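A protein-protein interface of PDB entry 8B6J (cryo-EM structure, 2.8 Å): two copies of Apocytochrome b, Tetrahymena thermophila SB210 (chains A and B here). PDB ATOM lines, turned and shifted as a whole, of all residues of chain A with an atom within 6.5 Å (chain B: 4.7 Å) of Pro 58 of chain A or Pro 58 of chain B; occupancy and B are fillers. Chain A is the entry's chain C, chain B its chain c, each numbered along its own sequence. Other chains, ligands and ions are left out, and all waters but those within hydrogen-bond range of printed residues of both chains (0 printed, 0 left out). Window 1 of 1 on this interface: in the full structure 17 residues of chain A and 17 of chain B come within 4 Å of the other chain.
Printed residues of chain B within 4 Å of Val 57 of chain A: Val 57 (3.8 Å), Thr 175 (3.8 Å) and Ile 179 (3.9 Å).
Pro 58 of chain A touches one residue of chain B.
Cys 138 of chain A touches none of the printed residues of chain B.
Printed residues of chain B within 4 Å of Thr 175 of chain A: Val 57 (3.8 Å).
Pro 58 of chain B touches one residue of chain A.
Of the printed residues of chain A, Thr 175 of chain B touches Val 57.
Of the printed residues of chain A, Ile 179 of chain B touches Val 57 (3.9 Å).
The nearest printed residue of chain B that does not touch Pro 58 of chain A is Val 57 of chain B (4.8 Å).
The nearest residue of chain A that does not touch Pro 58 of chain B is Val 57 of chain A (4.5 Å).
The nearest printed residue of chain A that does not touch Thr 175 of chain B is Leu 56 of chain A (6.9 Å).
Hydrophobic or aromatic side chains of chain A that line the printed part of chain B: Val 57, Pro 58 and Ile 179.
Among the printed residues, 6 pairs touch across the chains.
Among the printed residues, pairs that only touch across the chains: Pro 58 of chain A with Pro 58 of chain B, Val 57 of chain A with Val 57 of chain B, Val 57 of chain A with Thr 175 of chain B, Thr 175 of chain A with Val 57 of chain B, Val 57 of chain A with Ile 179 of chain B and Ile 179 of chain A with Val 57 of chain B.
Val 57 of chain A touches its own counterpart, Val 57 of chain B.
Val 57 of chain A touches Thr 175 of chain B, and with the chains exchanged Thr 175 of chain A touches Val 57 of chain B.
Val 57 of chain A touches Ile 179 of chain B, and with the chains exchanged Ile 179 of chain A touches Val 57 of chain B.
Pro 58 of chain A touches its own counterpart, Pro 58 of chain B.
Of the 6 pairs that touch across the chains among the printed residues, 6 have their exchanged pair printed and touching as well.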
ATOM      1  N   LEU A  56     -13.093 -10.194  -6.671  1.00  0.00           N
ATOM      2  CA  LEU A  56     -14.154  -9.293  -6.246  1.00  0.00           C
ATOM      3  C   LEU A  56     -15.375  -9.460  -7.142  1.00  0.00           C
ATOM      4  O   LEU A  56     -15.291  -9.267  -8.360  1.00  0.00           O
ATOM      5  CB  LEU A  56     -13.664  -7.846  -6.271  1.00  0.00           C
ATOM      6  CG  LEU A  56     -14.703  -6.784  -5.911  1.00  0.00           C
ATOM      7  CD1 LEU A  56     -14.115  -5.771  -4.952  1.00  0.00           C
ATOM      8  CD2 LEU A  56     -15.214  -6.094  -7.161  1.00  0.00           C
ATOM      9  N   VAL A  57     -16.502  -9.818  -6.537  1.00  0.00           N
ATOM     10  CA  VAL A  57     -17.792  -9.825  -7.218  1.00  0.00           C
ATOM     11  C   VAL A  57     -18.430  -8.453  -7.009  1.00  0.00           C
ATOM     12  O   VAL A  57     -18.625  -8.048  -5.853  1.00  0.00           O
ATOM     13  CB  VAL A  57     -18.703 -10.938  -6.689  1.00  0.00           C
ATOM     14  CG1 VAL A  57     -20.066 -10.871  -7.360  1.00  0.00           C
ATOM     15  CG2 VAL A  57     -18.065 -12.297  -6.915  1.00  0.00           C
ATOM     16  N   PRO A  58     -18.774  -7.721  -8.072  1.00  0.00           N
ATOM     17  CA  PRO A  58     -19.207  -6.325  -7.901  1.00  0.00           C
ATOM     18  C   PRO A  58     -20.516  -6.149  -7.142  1.00  0.00           C
ATOM     19  O   PRO A  58     -20.990  -5.013  -7.032  1.00  0.00           O
ATOM     20  CB  PRO A  58     -19.339  -5.824  -9.347  1.00  0.00           C
ATOM     21  CG  PRO A  58     -19.544  -7.046 -10.159  1.00  0.00           C
ATOM     22  CD  PRO A  58     -18.748  -8.116  -9.491  1.00  0.00           C
ATOM     23  N   GLU A  59     -21.126  -7.203  -6.625  1.00  0.00           N
ATOM     24  CA  GLU A  59     -22.343  -7.033  -5.838  1.00  0.00           C
ATOM     25  C   GLU A  59     -22.002  -6.390  -4.498  1.00  0.00           C
ATOM     26  O   GLU A  59     -21.187  -6.944  -3.749  1.00  0.00           O
ATOM     27  CB  GLU A  59     -23.029  -8.374  -5.622  1.00  0.00           C
ATOM     28  CG  GLU A  59     -24.390  -8.254  -4.969  1.00  0.00           C
ATOM     29  CD  GLU A  59     -25.186  -9.538  -5.048  1.00  0.00           C
ATOM     30  OE1 GLU A  59     -24.576 -10.602  -5.272  1.00  0.00           O
ATOM     31  OE2 GLU A  59     -26.423  -9.480  -4.892  1.00  0.00           O
ATOM     32  N   PRO A  60     -22.594  -5.244  -4.145  1.00  0.00           N
ATOM     33  CA  PRO A  60     -22.203  -4.584  -2.888  1.00  0.00           C
ATOM     34  C   PRO A  60     -22.399  -5.447  -1.656  1.00  0.00           C
ATOM     35  O   PRO A  60     -21.622  -5.328  -0.701  1.00  0.00           O
ATOM     36  CB  PRO A  60     -23.108  -3.344  -2.844  1.00  0.00           C
ATOM     37  CG  PRO A  60     -23.544  -3.124  -4.238  1.00  0.00           C
ATOM     38  CD  PRO A  60     -23.604  -4.467  -4.882  1.00  0.00           C
ATOM     39  N   MET A  61     -23.413  -6.306  -1.643  1.00  0.00           N
ATOM     40  CA  MET A  61     -23.734  -7.092  -0.459  1.00  0.00           C
ATOM     41  C   MET A  61     -22.864  -8.331  -0.310  1.00  0.00           C
ATOM     42  O   MET A  61     -22.987  -9.033   0.701  1.00  0.00           O
ATOM     43  CB  MET A  61     -25.207  -7.505  -0.495  1.00  0.00           C
ATOM     44  CG  MET A  61     -26.174  -6.332  -0.486  1.00  0.00           C
ATOM     45  SD  MET A  61     -26.092  -5.373   1.037  1.00  0.00           S
ATOM     46  CE  MET A  61     -27.436  -4.219   0.782  1.00  0.00           C
ATOM     47  N   ILE A  63     -19.262  -8.187  -1.493  1.00  0.00           N
ATOM     48  CA  ILE A  63     -17.842  -7.838  -1.546  1.00  0.00           C
ATOM     49  C   ILE A  63     -17.151  -8.091  -0.212  1.00  0.00           C
ATOM     50  O   ILE A  63     -16.084  -8.725  -0.205  1.00  0.00           O
ATOM     51  CB  ILE A  63     -17.672  -6.391  -2.040  1.00  0.00           C
ATOM     52  CG1 ILE A  63     -17.939  -6.325  -3.546  1.00  0.00           C
ATOM     53  CG2 ILE A  63     -16.275  -5.880  -1.713  1.00  0.00           C
ATOM     54  CD1 ILE A  63     -18.165  -4.931  -4.082  1.00  0.00           C
ATOM     55  N   CYS A 138     -16.545  -0.683  -0.647  1.00  0.00           N
ATOM     56  CA  CYS A 138     -17.879  -0.849  -0.068  1.00  0.00           C
ATOM     57  C   CYS A 138     -17.875  -0.639   1.442  1.00  0.00           C
ATOM     58  O   CYS A 138     -18.641  -1.273   2.171  1.00  0.00           O
ATOM     59  CB  CYS A 138     -18.465  -2.220  -0.414  1.00  0.00           C
ATOM     60  SG  CYS A 138     -18.949  -2.388  -2.143  1.00  0.00           S
ATOM     61  N   ASN A 174     -24.619   0.889  -5.246  1.00  0.00           N
ATOM     62  CA  ASN A 174     -25.506  -0.225  -5.542  1.00  0.00           C
ATOM     63  C   ASN A 174     -24.853  -1.071  -6.627  1.00  0.00           C
ATOM     64  O   ASN A 174     -23.728  -0.800  -7.059  1.00  0.00           O
ATOM     65  CB  ASN A 174     -26.895   0.273  -5.962  1.00  0.00           C
ATOM     66  CG  ASN A 174     -26.830   1.422  -6.945  1.00  0.00           C
ATOM     67  OD1 ASN A 174     -25.824   1.614  -7.626  1.00  0.00           O
ATOM     68  ND2 ASN A 174     -27.903   2.198  -7.022  1.00  0.00           N
ATOM     69  N   THR A 175     -25.560  -2.107  -7.077  1.00  0.00           N
ATOM     70  CA  THR A 175     -24.968  -3.033  -8.035  1.00  0.00           C
ATOM     71  C   THR A 175     -24.540  -2.308  -9.306  1.00  0.00           C
ATOM     72  O   THR A 175     -23.433  -2.523  -9.814  1.00  0.00           O
ATOM     73  CB  THR A 175     -25.956  -4.153  -8.357  1.00  0.00           C
ATOM     74  OG1 THR A 175     -26.338  -4.817  -7.146  1.00  0.00           O
ATOM     75  CG2 THR A 175     -25.328  -5.163  -9.303  1.00  0.00           C
ATOM     76  N   ASP A 176     -25.400  -1.431  -9.827  1.00  0.00           N
ATOM     77  CA  ASP A 176     -25.071  -0.713 -11.055  1.00  0.00           C
ATOM     78  C   ASP A 176     -23.842   0.166 -10.865  1.00  0.00           C
ATOM     79  O   ASP A 176     -22.890   0.113 -11.657  1.00  0.00           O
ATOM     80  CB  ASP A 176     -26.265   0.132 -11.498  1.00  0.00           C
ATOM     81  CG  ASP A 176     -27.503  -0.698 -11.758  1.00  0.00           C
ATOM     82  OD1 ASP A 176     -27.367  -1.828 -12.273  1.00  0.00           O
ATOM     83  OD2 ASP A 176     -28.614  -0.221 -11.447  1.00  0.00           O
ATOM     84  N   ILE A 178     -21.495   0.072  -8.542  1.00  0.00           N
ATOM     85  CA  ILE A 178     -20.283  -0.687  -8.253  1.00  0.00           C
ATOM     86  C   ILE A 178     -19.744  -1.334  -9.519  1.00  0.00           C
ATOM     87  O   ILE A 178     -18.539  -1.292  -9.784  1.00  0.00           O
ATOM     88  CB  ILE A 178     -20.545  -1.730  -7.152  1.00  0.00           C
ATOM     89  CG1 ILE A 178     -20.792  -1.046  -5.805  1.00  0.00           C
ATOM     90  CG2 ILE A 178     -19.370  -2.688  -7.043  1.00  0.00           C
ATOM     91  CD1 ILE A 178     -19.636  -0.196  -5.305  1.00  0.00           C
ATOM     92  N   ILE A 179     -20.618  -1.944 -10.323  1.00  0.00           N
ATOM     93  CA  ILE A 179     -20.155  -2.600 -11.543  1.00  0.00           C
ATOM     94  C   ILE A 179     -19.490  -1.589 -12.466  1.00  0.00           C
ATOM     95  O   ILE A 179     -18.369  -1.801 -12.954  1.00  0.00           O
ATOM     96  CB  ILE A 179     -21.324  -3.315 -12.244  1.00  0.00           C
ATOM     97  CG1 ILE A 179     -21.777  -4.521 -11.421  1.00  0.00           C
ATOM     98  CG2 ILE A 179     -20.912  -3.751 -13.640  1.00  0.00           C
ATOM     99  CD1 ILE A 179     -23.069  -5.140 -11.897  1.00  0.00           C
ATOM    100  N   ARG A 180     -20.172  -0.468 -12.720  1.00  0.00           N
ATOM    101  CA  ARG A 180     -19.631   0.517 -13.650  1.00  0.00           C
ATOM    102  C   ARG A 180     -18.310   1.081 -13.146  1.00  0.00           C
ATOM    103  O   ARG A 180     -17.342   1.193 -13.909  1.00  0.00           O
ATOM    104  CB  ARG A 180     -20.646   1.635 -13.873  1.00  0.00           C
ATOM    105  CG  ARG A 180     -21.946   1.158 -14.487  1.00  0.00           C
ATOM    106  CD  ARG A 180     -22.992   2.253 -14.505  1.00  0.00           C
ATOM    107  NE  ARG A 180     -24.292   1.746 -14.926  1.00  0.00           N
ATOM    108  CZ  ARG A 180     -25.396   2.477 -14.993  1.00  0.00           C
ATOM    109  NH1 ARG A 180     -25.395   3.761 -14.674  1.00  0.00           N
ATOM    110  NH2 ARG A 180     -26.529   1.906 -15.388  1.00  0.00           N
ATOM    111  N   ALA A 182     -16.155  -0.254 -11.007  1.00  0.00           N
ATOM    112  CA  ALA A 182     -15.096  -1.257 -11.017  1.00  0.00           C
ATOM    113  C   ALA A 182     -14.534  -1.447 -12.420  1.00  0.00           C
ATOM    114  O   ALA A 182     -13.311  -1.486 -12.616  1.00  0.00           O
ATOM    115  CB  ALA A 182     -15.627  -2.580 -10.468  1.00  0.00           C
ATOM    116  N   TYR A 183     -15.414  -1.579 -13.415  1.00  0.00           N
ATOM    117  CA  TYR A 183     -14.926  -1.776 -14.775  1.00  0.00           C
ATOM    118  C   TYR A 183     -14.157  -0.556 -15.264  1.00  0.00           C
ATOM    119  O   TYR A 183     -13.102  -0.691 -15.902  1.00  0.00           O
ATOM    120  CB  TYR A 183     -16.089  -2.105 -15.709  1.00  0.00           C
ATOM    121  CG  TYR A 183     -16.735  -3.453 -15.447  1.00  0.00           C
ATOM    122  CD1 TYR A 183     -16.136  -4.388 -14.610  1.00  0.00           C
ATOM    123  CD2 TYR A 183     -17.940  -3.790 -16.042  1.00  0.00           C
ATOM    124  CE1 TYR A 183     -16.721  -5.612 -14.374  1.00  0.00           C
ATOM    125  CE2 TYR A 183     -18.532  -5.013 -15.810  1.00  0.00           C
ATOM    126  CZ  TYR A 183     -17.918  -5.920 -14.976  1.00  0.00           C
ATOM    127  OH  TYR A 183     -18.505  -7.142 -14.742  1.00  0.00           O
ATOM    128  N   LEU B  56     -24.727  -7.857 -16.015  1.00  0.00           N
ATOM    129  CA  LEU B  56     -24.372  -9.227 -15.665  1.00  0.00           C
ATOM    130  C   LEU B  56     -23.435  -9.237 -14.464  1.00  0.00           C
ATOM    131  O   LEU B  56     -22.306  -8.741 -14.544  1.00  0.00           O
ATOM    132  CB  LEU B  56     -23.726  -9.927 -16.858  1.00  0.00           C
ATOM    133  CG  LEU B  56     -23.170 -11.327 -16.580  1.00  0.00           C
ATOM    134  CD1 LEU B  56     -23.572 -12.298 -17.673  1.00  0.00           C
ATOM    135  CD2 LEU B  56     -21.659 -11.283 -16.446  1.00  0.00           C
ATOM    136  N   VAL B  57     -23.905  -9.798 -13.355  1.00  0.00           N
ATOM    137  CA  VAL B  57     -23.062 -10.061 -12.192  1.00  0.00           C
ATOM    138  C   VAL B  57     -22.421 -11.429 -12.405  1.00  0.00           C
ATOM    139  O   VAL B  57     -23.138 -12.408 -12.659  1.00  0.00           O
ATOM    140  CB  VAL B  57     -23.869 -10.007 -10.885  1.00  0.00           C
ATOM    141  CG1 VAL B  57     -22.988 -10.364  -9.698  1.00  0.00           C
ATOM    142  CG2 VAL B  57     -24.476  -8.629 -10.700  1.00  0.00           C
ATOM    143  N   PRO B  58     -21.095 -11.555 -12.313  1.00  0.00           N
ATOM    144  CA  PRO B  58     -20.444 -12.799 -12.745  1.00  0.00           C
ATOM    145  C   PRO B  58     -20.638 -13.979 -11.802  1.00  0.00           C
ATOM    146  O   PRO B  58     -19.983 -15.011 -11.974  1.00  0.00           O
ATOM    147  CB  PRO B  58     -18.968 -12.400 -12.837  1.00  0.00           C
ATOM    148  CG  PRO B  58     -18.818 -11.303 -11.856  1.00  0.00           C
ATOM    149  CD  PRO B  58     -20.115 -10.549 -11.866  1.00  0.00           C
ATOM    150  N   GLU B  59     -21.507 -13.858 -10.810  1.00  0.00           N
ATOM    151  CA  GLU B  59     -21.787 -15.005  -9.954  1.00  0.00           C
ATOM    152  C   GLU B  59     -22.759 -15.952 -10.654  1.00  0.00           C
ATOM    153  O   GLU B  59     -23.826 -15.514 -11.096  1.00  0.00           O
ATOM    154  CB  GLU B  59     -22.364 -14.563  -8.617  1.00  0.00           C
ATOM    155  CG  GLU B  59     -22.678 -15.727  -7.691  1.00  0.00           C
ATOM    156  CD  GLU B  59     -22.712 -15.329  -6.233  1.00  0.00           C
ATOM    157  OE1 GLU B  59     -22.468 -14.143  -5.930  1.00  0.00           O
ATOM    158  OE2 GLU B  59     -22.979 -16.208  -5.386  1.00  0.00           O
ATOM    159  N   PRO B  60     -22.434 -17.243 -10.775  1.00  0.00           N
ATOM    160  CA  PRO B  60     -23.313 -18.140 -11.547  1.00  0.00           C
ATOM    161  C   PRO B  60     -24.735 -18.211 -11.024  1.00  0.00           C
ATOM    162  O   PRO B  60     -25.677 -18.310 -11.819  1.00  0.00           O
ATOM    163  CB  PRO B  60     -22.613 -19.503 -11.436  1.00  0.00           C
ATOM    164  CG  PRO B  60     -21.231 -19.212 -11.004  1.00  0.00           C
ATOM    165  CD  PRO B  60     -21.283 -17.961 -10.205  1.00  0.00           C
ATOM    166  N   ILE B  63     -26.873 -14.953 -12.226  1.00  0.00           N
ATOM    167  CA  ILE B  63     -26.999 -14.528 -13.621  1.00  0.00           C
ATOM    168  C   ILE B  63     -28.401 -14.772 -14.165  1.00  0.00           C
ATOM    169  O   ILE B  63     -28.967 -13.858 -14.784  1.00  0.00           O
ATOM    170  CB  ILE B  63     -25.908 -15.199 -14.475  1.00  0.00           C
ATOM    171  CG1 ILE B  63     -24.554 -14.543 -14.196  1.00  0.00           C
ATOM    172  CG2 ILE B  63     -26.258 -15.103 -15.954  1.00  0.00           C
ATOM    173  CD1 ILE B  63     -23.365 -15.341 -14.680  1.00  0.00           C
ATOM    174  N   THR B 175     -17.922 -19.317  -9.567  1.00  0.00           N
ATOM    175  CA  THR B 175     -17.654 -17.884  -9.488  1.00  0.00           C
ATOM    176  C   THR B 175     -16.317 -17.541 -10.134  1.00  0.00           C
ATOM    177  O   THR B 175     -16.229 -16.621 -10.957  1.00  0.00           O
ATOM    178  CB  THR B 175     -17.687 -17.428  -8.030  1.00  0.00           C
ATOM    179  OG1 THR B 175     -18.934 -17.806  -7.437  1.00  0.00           O
ATOM    180  CG2 THR B 175     -17.528 -15.920  -7.940  1.00  0.00           C
ATOM    181  N   ILE B 178     -16.393 -18.201 -14.015  1.00  0.00           N
ATOM    182  CA  ILE B 178     -17.249 -17.241 -14.702  1.00  0.00           C
ATOM    183  C   ILE B 178     -16.589 -15.871 -14.736  1.00  0.00           C
ATOM    184  O   ILE B 178     -16.590 -15.198 -15.771  1.00  0.00           O
ATOM    185  CB  ILE B 178     -18.639 -17.182 -14.042  1.00  0.00           C
ATOM    186  CG1 ILE B 178     -19.407 -18.486 -14.278  1.00  0.00           C
ATOM    187  CG2 ILE B 178     -19.433 -16.005 -14.586  1.00  0.00           C
ATOM    188  CD1 ILE B 178     -19.762 -18.760 -15.729  1.00  0.00           C
ATOM    189  N   ILE B 179     -16.017 -15.431 -13.613  1.00  0.00           N
ATOM    190  CA  ILE B 179     -15.382 -14.115 -13.579  1.00  0.00           C
ATOM    191  C   ILE B 179     -14.237 -14.055 -14.583  1.00  0.00           C
ATOM    192  O   ILE B 179     -14.142 -13.125 -15.398  1.00  0.00           O
ATOM    193  CB  ILE B 179     -14.897 -13.790 -12.156  1.00  0.00           C
ATOM    194  CG1 ILE B 179     -16.087 -13.607 -11.215  1.00  0.00           C
ATOM    195  CG2 ILE B 179     -14.042 -12.533 -12.162  1.00  0.00           C
ATOM    196  CD1 ILE B 179     -15.714 -13.592  -9.750  1.00  0.00           C
